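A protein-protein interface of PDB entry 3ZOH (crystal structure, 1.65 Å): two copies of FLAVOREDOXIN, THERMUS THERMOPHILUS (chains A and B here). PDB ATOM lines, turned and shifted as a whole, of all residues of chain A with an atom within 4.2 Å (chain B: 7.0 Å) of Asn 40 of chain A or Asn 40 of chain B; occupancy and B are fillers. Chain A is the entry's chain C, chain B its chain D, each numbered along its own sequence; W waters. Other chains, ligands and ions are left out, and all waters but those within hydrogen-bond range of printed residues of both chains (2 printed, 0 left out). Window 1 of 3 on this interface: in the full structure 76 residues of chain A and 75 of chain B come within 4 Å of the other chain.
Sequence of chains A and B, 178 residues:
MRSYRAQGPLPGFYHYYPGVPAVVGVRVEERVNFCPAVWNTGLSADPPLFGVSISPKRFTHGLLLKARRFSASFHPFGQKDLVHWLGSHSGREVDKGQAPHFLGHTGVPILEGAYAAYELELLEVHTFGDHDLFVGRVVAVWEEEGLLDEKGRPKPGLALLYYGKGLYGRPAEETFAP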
ATOM      1  N   VAL A  20      24.577  28.880  26.548  1.00  0.00           N
ATOM      2  CA  VAL A  20      25.050  29.906  27.452  1.00  0.00           C
ATOM      3  C   VAL A  20      23.979  30.995  27.505  1.00  0.00           C
ATOM      4  O   VAL A  20      23.586  31.517  26.458  1.00  0.00           O
ATOM      5  CB  VAL A  20      26.368  30.510  26.946  1.00  0.00           C
ATOM      6  CG1 VAL A  20      26.709  31.782  27.726  1.00  0.00           C
ATOM      7  CG2 VAL A  20      27.480  29.469  27.037  1.00  0.00           C
ATOM      8  N   ALA A  22      22.952  34.626  27.758  1.00  0.00           N
ATOM      9  CA  ALA A  22      23.494  35.979  27.719  1.00  0.00           C
ATOM     10  C   ALA A  22      22.645  36.809  28.658  1.00  0.00           C
ATOM     11  O   ALA A  22      21.423  36.741  28.601  1.00  0.00           O
ATOM     12  CB  ALA A  22      23.421  36.550  26.313  1.00  0.00           C
ATOM     13  N   ALA A  37      19.043  35.706  28.442  1.00  0.00           N
ATOM     14  CA  ALA A  37      18.529  35.311  27.143  1.00  0.00           C
ATOM     15  C   ALA A  37      19.344  34.148  26.586  1.00  0.00           C
ATOM     16  O   ALA A  37      20.442  34.350  26.087  1.00  0.00           O
ATOM     17  CB  ALA A  37      18.518  36.507  26.198  1.00  0.00           C
ATOM     18  N   VAL A  38      18.804  32.926  26.688  1.00  0.00           N
ATOM     19  CA  VAL A  38      19.463  31.750  26.118  1.00  0.00           C
ATOM     20  C   VAL A  38      19.314  31.705  24.584  1.00  0.00           C
ATOM     21  O   VAL A  38      20.134  31.080  23.873  1.00  0.00           O
ATOM     22  CB  VAL A  38      19.007  30.425  26.801  1.00  0.00           C
ATOM     23  CG1 VAL A  38      17.570  30.090  26.446  1.00  0.00           C
ATOM     24  CG2 VAL A  38      19.942  29.267  26.442  1.00  0.00           C
ATOM     25  N   TRP A  39      18.300  32.403  24.067  1.00  0.00           N
ATOM     26  CA  TRP A  39      18.148  32.500  22.613  1.00  0.00           C
ATOM     27  C   TRP A  39      19.038  33.631  22.159  1.00  0.00           C
ATOM     28  O   TRP A  39      18.621  34.787  22.091  1.00  0.00           O
ATOM     29  CB  TRP A  39      16.697  32.701  22.196  1.00  0.00           C
ATOM     30  CG  TRP A  39      15.874  31.484  22.334  1.00  0.00           C
ATOM     31  CD1 TRP A  39      16.266  30.260  22.836  1.00  0.00           C
ATOM     32  CD2 TRP A  39      14.480  31.369  22.039  1.00  0.00           C
ATOM     33  NE1 TRP A  39      15.195  29.387  22.842  1.00  0.00           N
ATOM     34  CE2 TRP A  39      14.089  30.043  22.356  1.00  0.00           C
ATOM     35  CE3 TRP A  39      13.522  32.256  21.523  1.00  0.00           C
ATOM     36  CZ2 TRP A  39      12.779  29.581  22.168  1.00  0.00           C
ATOM     37  CZ3 TRP A  39      12.208  31.799  21.361  1.00  0.00           C
ATOM     38  CH2 TRP A  39      11.854  30.472  21.678  1.00  0.00           C
ATOM     39  N   ASN A  40      20.294  33.281  21.932  1.00  0.00           N
ATOM     40  CA  ASN A  40      21.291  34.233  21.522  1.00  0.00           C
ATOM     41  C   ASN A  40      22.260  33.562  20.564  1.00  0.00           C
ATOM     42  O   ASN A  40      22.469  32.354  20.636  1.00  0.00           O
ATOM     43  CB  ASN A  40      22.009  34.862  22.737  1.00  0.00           C
ATOM     44  CG  ASN A  40      22.944  33.893  23.462  1.00  0.00           C
ATOM     45  OD1 ASN A  40      24.083  33.671  23.037  1.00  0.00           O
ATOM     46  ND2 ASN A  40      22.478  33.346  24.577  1.00  0.00           N
ATOM     47  N   THR A  41      22.837  34.340  19.660  1.00  0.00           N
ATOM     48  CA  THR A  41      23.826  33.788  18.745  1.00  0.00           C
ATOM     49  C   THR A  41      24.674  34.892  18.148  1.00  0.00           C
ATOM     50  O   THR A  41      24.204  36.023  17.979  1.00  0.00           O
ATOM     51  CB  THR A  41      23.170  32.965  17.603  1.00  0.00           C
ATOM     52  OG1 THR A  41      24.194  32.430  16.755  1.00  0.00           O
ATOM     53  CG2 THR A  41      22.233  33.828  16.753  1.00  0.00           C
ATOM     54  N   PHE A  50      25.896  40.504  17.181  1.00  0.00           N
ATOM     55  CA  PHE A  50      25.386  39.522  18.133  1.00  0.00           C
ATOM     56  C   PHE A  50      23.901  39.763  18.334  1.00  0.00           C
ATOM     57  O   PHE A  50      23.456  40.904  18.441  1.00  0.00           O
ATOM     58  CB  PHE A  50      26.159  39.652  19.457  1.00  0.00           C
ATOM     59  CG  PHE A  50      25.818  38.609  20.497  1.00  0.00           C
ATOM     60  CD1 PHE A  50      26.335  37.326  20.408  1.00  0.00           C
ATOM     61  CD2 PHE A  50      25.021  38.929  21.604  1.00  0.00           C
ATOM     62  CE1 PHE A  50      26.041  36.372  21.378  1.00  0.00           C
ATOM     63  CE2 PHE A  50      24.726  37.976  22.579  1.00  0.00           C
ATOM     64  CZ  PHE A  50      25.232  36.695  22.458  1.00  0.00           C
ATOM     65  N   GLY A  51      23.126  38.685  18.387  1.00  0.00           N
ATOM     66  CA  GLY A  51      21.692  38.825  18.509  1.00  0.00           C
ATOM     67  C   GLY A  51      21.109  38.134  19.714  1.00  0.00           C
ATOM     68  O   GLY A  51      21.624  37.114  20.174  1.00  0.00           O
ATOM     69  N   VAL A  52      20.046  38.728  20.237  1.00  0.00           N
ATOM     70  CA  VAL A  52      19.276  38.149  21.337  1.00  0.00           C
ATOM     71  C   VAL A  52      17.801  38.222  20.977  1.00  0.00           C
ATOM     72  O   VAL A  52      17.314  39.245  20.453  1.00  0.00           O
ATOM     73  CB  VAL A  52      19.572  38.825  22.700  1.00  0.00           C
ATOM     74  CG1 VAL A  52      20.997  38.522  23.127  1.00  0.00           C
ATOM     75  CG2 VAL A  52      19.312  40.338  22.649  1.00  0.00           C
ATOM     76  N   TYR B  16      30.816  34.162  23.967  1.00  0.00           N
ATOM     77  CA  TYR B  16      29.532  33.504  24.245  1.00  0.00           C
ATOM     78  C   TYR B  16      29.528  31.975  24.006  1.00  0.00           C
ATOM     79  O   TYR B  16      28.472  31.346  24.067  1.00  0.00           O
ATOM     80  CB  TYR B  16      28.461  34.164  23.373  1.00  0.00           C
ATOM     81  CG  TYR B  16      28.872  34.248  21.928  1.00  0.00           C
ATOM     82  CD1 TYR B  16      29.702  35.287  21.479  1.00  0.00           C
ATOM     83  CD2 TYR B  16      28.447  33.285  21.000  1.00  0.00           C
ATOM     84  CE1 TYR B  16      30.122  35.346  20.159  1.00  0.00           C
ATOM     85  CE2 TYR B  16      28.846  33.347  19.678  1.00  0.00           C
ATOM     86  CZ  TYR B  16      29.682  34.382  19.257  1.00  0.00           C
ATOM     87  OH  TYR B  16      30.073  34.463  17.935  1.00  0.00           O
ATOM     88  N   GLY B  19      28.826  26.459  22.332  1.00  0.00           N
ATOM     89  CA  GLY B  19      27.478  26.234  21.860  1.00  0.00           C
ATOM     90  C   GLY B  19      27.335  24.849  21.272  1.00  0.00           C
ATOM     91  O   GLY B  19      28.321  24.205  20.870  1.00  0.00           O
ATOM     92  N   VAL B  20      26.094  24.404  21.218  1.00  0.00           N
ATOM     93  CA  VAL B  20      25.716  23.225  20.467  1.00  0.00           C
ATOM     94  C   VAL B  20      25.787  23.543  18.962  1.00  0.00           C
ATOM     95  O   VAL B  20      25.117  24.474  18.493  1.00  0.00           O
ATOM     96  CB  VAL B  20      24.287  22.810  20.860  1.00  0.00           C
ATOM     97  CG1 VAL B  20      23.840  21.584  20.067  1.00  0.00           C
ATOM     98  CG2 VAL B  20      24.221  22.556  22.357  1.00  0.00           C
ATOM     99  N   PRO B  21      26.610  22.795  18.207  1.00  0.00           N
ATOM    100  CA  PRO B  21      26.567  22.914  16.750  1.00  0.00           C
ATOM    101  C   PRO B  21      25.332  22.214  16.209  1.00  0.00           C
ATOM    102  O   PRO B  21      25.034  21.081  16.595  1.00  0.00           O
ATOM    103  CB  PRO B  21      27.858  22.230  16.277  1.00  0.00           C
ATOM    104  CG  PRO B  21      28.291  21.357  17.415  1.00  0.00           C
ATOM    105  CD  PRO B  21      27.609  21.813  18.672  1.00  0.00           C
ATOM    106  N   ALA B  22      24.574  22.907  15.379  1.00  0.00           N
ATOM    107  CA  ALA B  22      23.452  22.288  14.696  1.00  0.00           C
ATOM    108  C   ALA B  22      24.029  21.794  13.393  1.00  0.00           C
ATOM    109  O   ALA B  22      24.680  22.562  12.692  1.00  0.00           O
ATOM    110  CB  ALA B  22      22.371  23.314  14.426  1.00  0.00           C
ATOM    111  N   VAL B  23      23.821  20.519  13.067  1.00  0.00           N
ATOM    112  CA  VAL B  23      24.210  20.052  11.744  1.00  0.00           C
ATOM    113  C   VAL B  23      23.094  20.362  10.745  1.00  0.00           C
ATOM    114  O   VAL B  23      21.966  19.895  10.906  1.00  0.00           O
ATOM    115  CB  VAL B  23      24.593  18.559  11.724  1.00  0.00           C
ATOM    116  CG1 VAL B  23      24.856  18.114  10.292  1.00  0.00           C
ATOM    117  CG2 VAL B  23      25.821  18.305  12.597  1.00  0.00           C
ATOM    118  N   VAL B  24      23.435  21.160   9.729  1.00  0.00           N
ATOM    119  CA  VAL B  24      22.468  21.625   8.746  1.00  0.00           C
ATOM    120  C   VAL B  24      22.544  20.706   7.532  1.00  0.00           C
ATOM    121  O   VAL B  24      23.553  20.666   6.828  1.00  0.00           O
ATOM    122  CB  VAL B  24      22.732  23.108   8.357  1.00  0.00           C
ATOM    123  CG1 VAL B  24      21.790  23.575   7.244  1.00  0.00           C
ATOM    124  CG2 VAL B  24      22.580  24.010   9.569  1.00  0.00           C
ATOM    125  N   ALA B  37      26.665  24.296  12.199  1.00  0.00           N
ATOM    126  CA  ALA B  37      26.413  25.703  12.429  1.00  0.00           C
ATOM    127  C   ALA B  37      26.324  25.963  13.933  1.00  0.00           C
ATOM    128  O   ALA B  37      25.307  25.686  14.549  1.00  0.00           O
ATOM    129  CB  ALA B  37      25.133  26.140  11.703  1.00  0.00           C
ATOM    130  N   VAL B  38      27.392  26.510  14.521  1.00  0.00           N
ATOM    131  CA  VAL B  38      27.348  26.888  15.934  1.00  0.00           C
ATOM    132  C   VAL B  38      26.537  28.184  16.148  1.00  0.00           C
ATOM    133  O   VAL B  38      26.017  28.449  17.243  1.00  0.00           O
ATOM    134  CB  VAL B  38      28.762  26.967  16.565  1.00  0.00           C
ATOM    135  CG1 VAL B  38      29.495  28.211  16.090  1.00  0.00           C
ATOM    136  CG2 VAL B  38      28.668  26.929  18.093  1.00  0.00           C
ATOM    137  N   TRP B  39      26.404  28.988  15.096  1.00  0.00           N
ATOM    138  CA  TRP B  39      25.539  30.148  15.203  1.00  0.00           C
ATOM    139  C   TRP B  39      24.131  29.698  14.895  1.00  0.00           C
ATOM    140  O   TRP B  39      23.711  29.654  13.741  1.00  0.00           O
ATOM    141  CB  TRP B  39      25.990  31.288  14.300  1.00  0.00           C
ATOM    142  CG  TRP B  39      27.283  31.896  14.711  1.00  0.00           C
ATOM    143  CD1 TRP B  39      28.057  31.593  15.828  1.00  0.00           C
ATOM    144  CD2 TRP B  39      27.976  32.922  14.017  1.00  0.00           C
ATOM    145  NE1 TRP B  39      29.186  32.379  15.843  1.00  0.00           N
ATOM    146  CE2 TRP B  39      29.160  33.205  14.749  1.00  0.00           C
ATOM    147  CE3 TRP B  39      27.710  33.645  12.850  1.00  0.00           C
ATOM    148  CZ2 TRP B  39      30.073  34.172  14.344  1.00  0.00           C
ATOM    149  CZ3 TRP B  39      28.636  34.614  12.449  1.00  0.00           C
ATOM    150  CH2 TRP B  39      29.796  34.858  13.191  1.00  0.00           C
ATOM    151  N   ASN B  40      23.437  29.298  15.950  1.00  0.00           N
ATOM    152  CA  ASN B  40      22.077  28.835  15.827  1.00  0.00           C
ATOM    153  C   ASN B  40      21.332  29.195  17.085  1.00  0.00           C
ATOM    154  O   ASN B  40      21.934  29.306  18.161  1.00  0.00           O
ATOM    155  CB  ASN B  40      22.018  27.323  15.556  1.00  0.00           C
ATOM    156  CG  ASN B  40      22.370  26.489  16.780  1.00  0.00           C
ATOM    157  OD1 ASN B  40      21.554  26.334  17.692  1.00  0.00           O
ATOM    158  ND2 ASN B  40      23.575  25.937  16.793  1.00  0.00           N
ATOM    159  N   THR B  41      20.020  29.347  16.963  1.00  0.00           N
ATOM    160  CA  THR B  41      19.189  29.602  18.138  1.00  0.00           C
ATOM    161  C   THR B  41      17.726  29.362  17.846  1.00  0.00           C
ATOM    162  O   THR B  41      17.284  29.469  16.703  1.00  0.00           O
ATOM    163  CB  THR B  41      19.372  31.040  18.685  1.00  0.00           C
ATOM    164  OG1 THR B  41      18.566  31.209  19.865  1.00  0.00           O
ATOM    165  CG2 THR B  41      18.957  32.093  17.633  1.00  0.00           C
ATOM    166  N   GLY B  42      16.979  29.031  18.891  1.00  0.00           N
ATOM    167  CA  GLY B  42      15.520  29.158  18.851  1.00  0.00           C
ATOM    168  C   GLY B  42      15.141  30.599  18.551  1.00  0.00           C
ATOM    169  O   GLY B  42      15.839  31.536  18.950  1.00  0.00           O
ATOM    170  N   PHE B  50      13.370  28.298  14.295  1.00  0.00           N
ATOM    171  CA  PHE B  50      14.738  28.006  14.645  1.00  0.00           C
ATOM    172  C   PHE B  50      15.604  28.587  13.547  1.00  0.00           C
ATOM    173  O   PHE B  50      15.338  28.369  12.361  1.00  0.00           O
ATOM    174  CB  PHE B  50      14.903  26.477  14.737  1.00  0.00           C
ATOM    175  CG  PHE B  50      16.277  26.023  15.152  1.00  0.00           C
ATOM    176  CD1 PHE B  50      16.652  26.067  16.487  1.00  0.00           C
ATOM    177  CD2 PHE B  50      17.195  25.532  14.211  1.00  0.00           C
ATOM    178  CE1 PHE B  50      17.916  25.656  16.884  1.00  0.00           C
ATOM    179  CE2 PHE B  50      18.471  25.124  14.606  1.00  0.00           C
ATOM    180  CZ  PHE B  50      18.824  25.183  15.954  1.00  0.00           C
ATOM    181  N   GLY B  51      16.633  29.329  13.945  1.00  0.00           N
ATOM    182  CA  GLY B  51      17.551  29.946  13.011  1.00  0.00           C
ATOM    183  C   GLY B  51      18.942  29.366  12.973  1.00  0.00           C
ATOM    184  O   GLY B  51      19.485  28.964  14.005  1.00  0.00           O
ATOM    185  N   VAL B  52      19.502  29.308  11.766  1.00  0.00           N
ATOM    186  CA  VAL B  52      20.921  29.036  11.580  1.00  0.00           C
ATOM    187  C   VAL B  52      21.525  30.160  10.754  1.00  0.00           C
ATOM    188  O   VAL B  52      20.921  30.634   9.779  1.00  0.00           O
ATOM    189  CB  VAL B  52      21.179  27.656  10.943  1.00  0.00           C
ATOM    190  CG1 VAL B  52      20.712  26.547  11.889  1.00  0.00           C
ATOM    191  CG2 VAL B  52      20.490  27.534   9.586  1.00  0.00           C
ATOM    192  N   SER B  53      22.707  30.609  11.159  1.00  0.00           N
ATOM    193  CA  SER B  53      23.376  31.703  10.463  1.00  0.00           C
ATOM    194  C   SER B  53      24.495  31.107   9.603  1.00  0.00           C
ATOM    195  O   SER B  53      25.429  30.501  10.126  1.00  0.00           O
ATOM    196  CB  SER B  53      23.906  32.710  11.480  1.00  0.00           C
ATOM    197  OG  SER B  53      24.602  33.767  10.841  1.00  0.00           O
ATOM    198  N   PHE B  74      21.168  17.355  16.058  1.00  0.00           N
ATOM    199  CA  PHE B  74      21.942  17.599  17.266  1.00  0.00           C
ATOM    200  C   PHE B  74      22.548  16.286  17.739  1.00  0.00           C
ATOM    201  O   PHE B  74      21.827  15.315  17.995  1.00  0.00           O
ATOM    202  CB  PHE B  74      21.034  18.268  18.313  1.00  0.00           C
ATOM    203  CG  PHE B  74      20.216  19.386  17.736  1.00  0.00           C
ATOM    204  CD1 PHE B  74      20.823  20.577  17.359  1.00  0.00           C
ATOM    205  CD2 PHE B  74      18.855  19.220  17.491  1.00  0.00           C
ATOM    206  CE1 PHE B  74      20.074  21.602  16.782  1.00  0.00           C
ATOM    207  CE2 PHE B  74      18.108  20.245  16.914  1.00  0.00           C
ATOM    208  CZ  PHE B  74      18.727  21.428  16.561  1.00  0.00           C
ATOM    209  N   LEU B 133      21.048  34.892   8.199  1.00  0.00           N
ATOM    210  CA  LEU B 133      20.209  34.089   9.097  1.00  0.00           C
ATOM    211  C   LEU B 133      19.084  33.428   8.323  1.00  0.00           C
ATOM    212  O   LEU B 133      18.242  34.121   7.725  1.00  0.00           O
ATOM    213  CB  LEU B 133      19.661  34.923  10.252  1.00  0.00           C
ATOM    214  CG  LEU B 133      18.925  34.171  11.359  1.00  0.00           C
ATOM    215  CD1 LEU B 133      19.823  33.173  12.081  1.00  0.00           C
ATOM    216  CD2 LEU B 133      18.338  35.161  12.350  1.00  0.00           C
HETATM  217  O   HOH W   1      26.436  31.193  18.741  1.00  0.00           O
HETATM  218  O   HOH W   2      19.066  28.944  21.530  1.00  0.00           O
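Trp 39 of chain A touches Thr 41 of chain B, and with the chains exchanged Thr 41 of chain A touches Trp 39 of chain B.
Asn 40 of chain A touches its own counterpart, Asn 40 of chain B.
Asn 40 of chain A touches Thr 41 of chain B, and with the chains exchanged Thr 41 of chain A touches Asn 40 of chain B.
Thr 41 of chain B touches its own counterpart, Thr 41 of chain A.
Of the 9 pairs that touch across the chains among the printed residues, 6 have their exchanged pair printed and touching as well.
Printed residues of chain B within 4 Å of Asn 40 of chain A: Asn 40 and Thr 41.
Asn 40 of chain B touches two residues of chain A.
Of the printed residues of chain A, Gly 42 of chain B touches Trp 39.
Of the printed residues of chain A, Tyr 16 of chain B touches Val 20 and Phe 50.
Of the printed residues of chain B, Trp 39 of chain A touches Thr 41 and Gly 42.
The nearest residue of chain B that does not touch Asn 40 of chain A is Tyr 16 of chain B (4.4 Å).
The nearest printed residue of chain A that does not touch Asn 40 of chain B is Val 38 of chain A (6.2 Å).
The side-chain hydroxyl of Thr 41 of chain B lies within hydrogen-bond range of the backbone NH of Asn 40 of chain A.
N of Asn 40 of chain B is in hydrogen-bond range of OG1 of Thr 41 of chain A, at 3.3 Å.
The backbone carbonyl oxygen (O) of Val 20 of chain B is in hydrogen-bond range of the side-chain amide nitrogen (ND2) of Asn 40 of chain B (2.7 Å).
The backbone carbonyl oxygen (O) of Ala 37 of chain B lies within hydrogen-bond range of the side-chain amide nitrogen (ND2) of Asn 40 of chain B (2.8 Å).
ND2 of Asn 40 of chain A is in hydrogen-bond range of O of Val 38 of chain A (3.3 Å).
The backbone carbonyl oxygen (O) of Val 20 of chain A lies within hydrogen-bond range of the side-chain amide nitrogen (ND2) of Asn 40 of chain A, 2.8 Å away.
The backbone carbonyl oxygen (O) of Ala 37 of chain A sits at hydrogen-bond distance from the side-chain amide nitrogen (ND2) of Asn 40 of chain A (2.7 Å).
The backbone carbonyl oxygen (O) of Trp 39 of chain B is in hydrogen-bond range of the backbone NH (N) of Ser 53 of chain B (2.9 Å).
Water W2 lies within hydrogen-bond range of OG1 of Thr 41 of chain B (2.9 Å), O of Val 38 of chain A (3.3 Å) and N of Gly 42 of chain B (3.4 Å).
Water W1 bridges O of Val 38 of chain B (3.2 Å) and OG1 of Thr 41 of chain A (3.2 Å).
Hydrophobic or aromatic side chains of chain B within 4 Å of the printed part of chain A: Tyr 16 and Trp 39.
Among the printed residues, no Asp or Glu carboxylate lies within 4 Å of a Lys or Arg side-chain nitrogen of the other chain.
Among the printed residues, merely in contact across the chains: Trp 39 of chain A with Thr 41 of chain B (3.1 Å), Thr 41 of chain A with Trp 39 of chain B (3.1 Å), Trp 39 of chain A with Gly 42 of chain B (3.4 Å), Phe 50 of chain A with Tyr 16 of chain B (3.6 Å), Val 20 of chain A with Tyr 16 of chain B (3.7 Å), Thr 41 of chain A with Thr 41 of chain B (3.8 Å) and Asn 40 of chain A with Asn 40 of chain B (3.96 Å).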
